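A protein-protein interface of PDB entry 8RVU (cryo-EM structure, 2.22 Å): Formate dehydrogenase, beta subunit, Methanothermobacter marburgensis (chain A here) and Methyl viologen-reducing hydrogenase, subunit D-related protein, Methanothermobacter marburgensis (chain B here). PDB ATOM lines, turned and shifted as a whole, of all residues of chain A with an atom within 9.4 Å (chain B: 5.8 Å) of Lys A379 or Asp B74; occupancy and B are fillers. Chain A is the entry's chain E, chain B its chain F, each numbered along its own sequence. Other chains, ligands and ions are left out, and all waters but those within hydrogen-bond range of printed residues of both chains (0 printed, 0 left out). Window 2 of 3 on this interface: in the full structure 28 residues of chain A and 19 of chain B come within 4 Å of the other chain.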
ATOM      1  N   PRO A 373       2.802  28.730  11.393  1.00  0.00           N
ATOM      2  CA  PRO A 373       2.292  27.643  10.543  1.00  0.00           C
ATOM      3  C   PRO A 373       1.324  28.125   9.472  1.00  0.00           C
ATOM      4  O   PRO A 373       1.079  27.421   8.488  1.00  0.00           O
ATOM      5  CB  PRO A 373       1.598  26.709  11.540  1.00  0.00           C
ATOM      6  CG  PRO A 373       2.244  26.985  12.845  1.00  0.00           C
ATOM      7  CD  PRO A 373       2.681  28.417  12.828  1.00  0.00           C
ATOM      8  N   SER A 376       3.164  28.001   6.183  1.00  0.00           N
ATOM      9  CA  SER A 376       3.882  26.795   5.799  1.00  0.00           C
ATOM     10  C   SER A 376       3.517  26.382   4.379  1.00  0.00           C
ATOM     11  O   SER A 376       2.356  26.461   3.968  1.00  0.00           O
ATOM     12  CB  SER A 376       3.567  25.658   6.770  1.00  0.00           C
ATOM     13  OG  SER A 376       4.229  24.467   6.382  1.00  0.00           O
ATOM     14  N   GLY A 377       4.523  25.938   3.626  1.00  0.00           N
ATOM     15  CA  GLY A 377       4.315  25.437   2.282  1.00  0.00           C
ATOM     16  C   GLY A 377       4.084  23.948   2.182  1.00  0.00           C
ATOM     17  O   GLY A 377       3.727  23.455   1.109  1.00  0.00           O
ATOM     18  N   GLU A 378       4.278  23.216   3.275  1.00  0.00           N
ATOM     19  CA  GLU A 378       4.109  21.773   3.268  1.00  0.00           C
ATOM     20  C   GLU A 378       2.634  21.405   3.388  1.00  0.00           C
ATOM     21  O   GLU A 378       1.784  22.228   3.739  1.00  0.00           O
ATOM     22  CB  GLU A 378       4.898  21.123   4.409  1.00  0.00           C
ATOM     23  CG  GLU A 378       6.276  21.727   4.685  1.00  0.00           C
ATOM     24  CD  GLU A 378       7.389  21.009   3.946  1.00  0.00           C
ATOM     25  OE1 GLU A 378       8.563  21.173   4.338  1.00  0.00           O
ATOM     26  OE2 GLU A 378       7.092  20.285   2.973  1.00  0.00           O
ATOM     27  N   LYS A 379       2.336  20.143   3.083  1.00  0.00           N
ATOM     28  CA  LYS A 379       0.988  19.608   3.209  1.00  0.00           C
ATOM     29  C   LYS A 379       0.613  19.285   4.651  1.00  0.00           C
ATOM     30  O   LYS A 379      -0.431  18.668   4.881  1.00  0.00           O
ATOM     31  CB  LYS A 379       0.838  18.353   2.345  1.00  0.00           C
ATOM     32  CG  LYS A 379       0.685  18.636   0.860  1.00  0.00           C
ATOM     33  CD  LYS A 379       0.069  17.452   0.130  1.00  0.00           C
ATOM     34  CE  LYS A 379       0.430  17.459  -1.345  1.00  0.00           C
ATOM     35  NZ  LYS A 379       0.370  18.825  -1.926  1.00  0.00           N
ATOM     36  N   ASP A 380       1.436  19.677   5.620  1.00  0.00           N
ATOM     37  CA  ASP A 380       1.134  19.438   7.027  1.00  0.00           C
ATOM     38  C   ASP A 380      -0.188  20.090   7.415  1.00  0.00           C
ATOM     39  O   ASP A 380      -0.503  21.191   6.965  1.00  0.00           O
ATOM     40  CB  ASP A 380       2.262  19.969   7.913  1.00  0.00           C
ATOM     41  CG  ASP A 380       2.327  21.485   7.928  1.00  0.00           C
ATOM     42  OD1 ASP A 380       2.972  22.063   7.030  1.00  0.00           O
ATOM     43  OD2 ASP A 380       1.730  22.100   8.837  1.00  0.00           O
ATOM     44  N   GLY B  69      -5.871  16.540  -0.107  1.00  0.00           N
ATOM     45  CA  GLY B  69      -5.208  15.643  -1.026  1.00  0.00           C
ATOM     46  C   GLY B  69      -5.760  15.669  -2.435  1.00  0.00           C
ATOM     47  O   GLY B  69      -5.175  15.033  -3.321  1.00  0.00           O
ATOM     48  N   ASP B  70      -6.861  16.384  -2.669  1.00  0.00           N
ATOM     49  CA  ASP B  70      -7.506  16.433  -3.977  1.00  0.00           C
ATOM     50  C   ASP B  70      -7.491  17.829  -4.587  1.00  0.00           C
ATOM     51  O   ASP B  70      -8.133  18.045  -5.622  1.00  0.00           O
ATOM     52  CB  ASP B  70      -8.950  15.935  -3.872  1.00  0.00           C
ATOM     53  CG  ASP B  70      -9.051  14.427  -3.927  1.00  0.00           C
ATOM     54  OD1 ASP B  70      -8.401  13.754  -3.099  1.00  0.00           O
ATOM     55  OD2 ASP B  70      -9.781  13.915  -4.800  1.00  0.00           O
ATOM     56  N   CYS B  71      -6.786  18.778  -3.979  1.00  0.00           N
ATOM     57  CA  CYS B  71      -6.742  20.132  -4.512  1.00  0.00           C
ATOM     58  C   CYS B  71      -6.153  20.127  -5.916  1.00  0.00           C
ATOM     59  O   CYS B  71      -5.143  19.467  -6.178  1.00  0.00           O
ATOM     60  CB  CYS B  71      -5.916  21.029  -3.590  1.00  0.00           C
ATOM     61  SG  CYS B  71      -5.522  22.657  -4.268  1.00  0.00           S
ATOM     62  N   HIS B  72      -6.791  20.868  -6.826  1.00  0.00           N
ATOM     63  CA  HIS B  72      -6.274  20.963  -8.186  1.00  0.00           C
ATOM     64  C   HIS B  72      -4.854  21.511  -8.191  1.00  0.00           C
ATOM     65  O   HIS B  72      -4.007  21.067  -8.976  1.00  0.00           O
ATOM     66  CB  HIS B  72      -7.191  21.842  -9.033  1.00  0.00           C
ATOM     67  CG  HIS B  72      -6.868  21.818 -10.494  1.00  0.00           C
ATOM     68  ND1 HIS B  72      -7.263  20.794 -11.328  1.00  0.00           N
ATOM     69  CD2 HIS B  72      -6.190  22.695 -11.270  1.00  0.00           C
ATOM     70  CE1 HIS B  72      -6.840  21.041 -12.555  1.00  0.00           C
ATOM     71  NE2 HIS B  72      -6.186  22.188 -12.547  1.00  0.00           N
ATOM     72  N   TYR B  73      -4.578  22.449  -7.336  1.00  0.00           N
ATOM     73  CA  TYR B  73      -3.374  23.246  -7.230  1.00  0.00           C
ATOM     74  C   TYR B  73      -2.525  22.676  -6.158  1.00  0.00           C
ATOM     75  O   TYR B  73      -1.791  23.336  -5.696  1.00  0.00           O
ATOM     76  CB  TYR B  73      -3.790  24.683  -7.047  1.00  0.00           C
ATOM     77  CG  TYR B  73      -4.631  25.266  -8.097  1.00  0.00           C
ATOM     78  CD1 TYR B  73      -4.035  25.730  -9.240  1.00  0.00           C
ATOM     79  CD2 TYR B  73      -5.976  25.411  -7.890  1.00  0.00           C
ATOM     80  CE1 TYR B  73      -4.797  26.309 -10.211  1.00  0.00           C
ATOM     81  CE2 TYR B  73      -6.742  26.024  -8.839  1.00  0.00           C
ATOM     82  CZ  TYR B  73      -6.144  26.433 -10.004  1.00  0.00           C
ATOM     83  OH  TYR B  73      -6.765  27.028 -11.004  1.00  0.00           O
ATOM     84  N   ASP B  74      -2.696  21.468  -5.846  1.00  0.00           N
ATOM     85  CA  ASP B  74      -1.971  20.626  -4.877  1.00  0.00           C
ATOM     86  C   ASP B  74      -2.208  20.854  -3.353  1.00  0.00           C
ATOM     87  O   ASP B  74      -2.623  19.973  -2.732  1.00  0.00           O
ATOM     88  CB  ASP B  74      -0.552  20.619  -5.443  1.00  0.00           C
ATOM     89  CG  ASP B  74       0.612  20.069  -4.698  1.00  0.00           C
ATOM     90  OD1 ASP B  74       0.956  18.941  -4.970  1.00  0.00           O
ATOM     91  OD2 ASP B  74       1.226  20.807  -3.964  1.00  0.00           O
ATOM     92  N   SER B  75      -2.006  22.028  -2.826  1.00  0.00           N
ATOM     93  CA  SER B  75      -2.029  22.289  -1.420  1.00  0.00           C
ATOM     94  C   SER B  75      -2.668  23.614  -1.081  1.00  0.00           C
ATOM     95  O   SER B  75      -2.437  23.967  -0.034  1.00  0.00           O
ATOM     96  CB  SER B  75      -0.674  22.225  -1.014  1.00  0.00           C
ATOM     97  OG  SER B  75       0.127  23.015  -1.854  1.00  0.00           O
ATOM     98  N   GLY B  76      -3.551  24.218  -1.816  1.00  0.00           N
ATOM     99  CA  GLY B  76      -4.266  25.413  -1.390  1.00  0.00           C
ATOM    100  C   GLY B  76      -5.206  25.166  -0.225  1.00  0.00           C
ATOM    101  O   GLY B  76      -5.306  25.988   0.695  1.00  0.00           O
ATOM    102  N   ASN B  77      -5.915  24.035  -0.247  1.00  0.00           N
ATOM    103  CA  ASN B  77      -6.921  23.784   0.778  1.00  0.00           C
ATOM    104  C   ASN B  77      -6.299  23.636   2.159  1.00  0.00           C
ATOM    105  O   ASN B  77      -6.960  23.921   3.159  1.00  0.00           O
ATOM    106  CB  ASN B  77      -7.746  22.546   0.420  1.00  0.00           C
ATOM    107  CG  ASN B  77      -6.891  21.358   0.029  1.00  0.00           C
ATOM    108  OD1 ASN B  77      -5.665  21.438   0.009  1.00  0.00           O
ATOM    109  ND2 ASN B  77      -7.541  20.247  -0.294  1.00  0.00           N
ATOM    110  N   TYR B  78      -5.035  23.217   2.245  1.00  0.00           N
ATOM    111  CA  TYR B  78      -4.354  23.199   3.537  1.00  0.00           C
ATOM    112  C   TYR B  78      -4.251  24.610   4.108  1.00  0.00           C
ATOM    113  O   TYR B  78      -4.546  24.854   5.289  1.00  0.00           O
ATOM    114  CB  TYR B  78      -2.960  22.595   3.378  1.00  0.00           C
ATOM    115  CG  TYR B  78      -2.948  21.139   2.977  1.00  0.00           C
ATOM    116  CD1 TYR B  78      -3.023  20.132   3.928  1.00  0.00           C
ATOM    117  CD2 TYR B  78      -2.851  20.774   1.642  1.00  0.00           C
ATOM    118  CE1 TYR B  78      -3.008  18.800   3.557  1.00  0.00           C
ATOM    119  CE2 TYR B  78      -2.834  19.448   1.263  1.00  0.00           C
ATOM    120  CZ  TYR B  78      -2.909  18.466   2.223  1.00  0.00           C
ATOM    121  OH  TYR B  78      -2.896  17.143   1.848  1.00  0.00           O
ATOM    122  N   ARG B  82      -6.004  26.177   7.586  1.00  0.00           N
ATOM    123  CA  ARG B  82      -5.354  26.952   8.641  1.00  0.00           C
ATOM    124  C   ARG B  82      -6.066  28.288   8.847  1.00  0.00           C
ATOM    125  O   ARG B  82      -6.393  28.677   9.983  1.00  0.00           O
ATOM    126  CB  ARG B  82      -3.883  27.175   8.293  1.00  0.00           C
ATOM    127  CG  ARG B  82      -3.083  25.897   8.100  1.00  0.00           C
ATOM    128  CD  ARG B  82      -1.638  26.201   7.743  1.00  0.00           C
ATOM    129  NE  ARG B  82      -1.037  25.147   6.934  1.00  0.00           N
ATOM    130  CZ  ARG B  82      -0.243  25.349   5.889  1.00  0.00           C
ATOM    131  NH1 ARG B  82       0.093  26.567   5.494  1.00  0.00           N
ATOM    132  NH2 ARG B  82       0.230  24.300   5.224  1.00  0.00           N
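O of Glu A378 lies within hydrogen-bond range of NH2 of Arg B82 (3.0 Å). NH2 of Arg B82 is in salt-bridge range of OD1 of Asp A380, at 3.97 Å. NH1 of Arg B82 sits close to O of Pro A373, 3.3 Å away. The backbone carbonyl oxygen (O) of Ser A376 lies within hydrogen-bond range of the guanidinium group (NH1) of Arg B82 (2.7 Å). The side-chain amino group (NZ) of Lys A379 lies within salt-bridge range of the side-chain carboxylate (OD2) of Asp B74.
OG of Ser A376 lies within hydrogen-bond range of N of Glu A378, at 3.3 Å. The side-chain carboxylate (OD1) of Asp A380 is in hydrogen-bond range of the side-chain hydroxyl (OG) of Ser A376, 2.8 Å away. SG of Cys B71 lies close to N of Asp B74. OG of Ser B75 is in hydrogen-bond range of OD2 of Asp B74 (3.2 Å).
NZ of Lys A379 touches CB of Ser B75 (3.7 Å). O of Lys A379 touches CE1 of Tyr B78, 2.9 Å away.
Printed residues of chain B within 4 Å of Pro A373: Arg B82. Of the printed residues of chain B, Glu A378 touches Arg B82. Lys A379 touches just these residues of chain B: Asp B74 (3.0 Å), Ser B75 (3.7 Å) and Tyr B78 (2.9 Å). No residue of chain A comes within 4 Å of Cys B71. Asp B74 touches just one residue of chain A: Lys A379. Of chain A, only Lys A379 (3.7 Å) comes within 4 Å of Ser B75. Gly B76 touches none of the printed residues of chain A. Printed residues of chain A within 4 Å of Tyr B78: Lys A379. Printed residues of chain A within 4 Å of Arg B82: Pro A373 (3.1 Å), Ser A376 (2.7 Å), Glu A378 (3.0 Å) and Asp A380 (3.6 Å). The nearest printed residue of chain A that does not touch Arg B82 is Gly A377 (4.8 Å).
Among the printed residues, 7 pairs touch across the chains.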
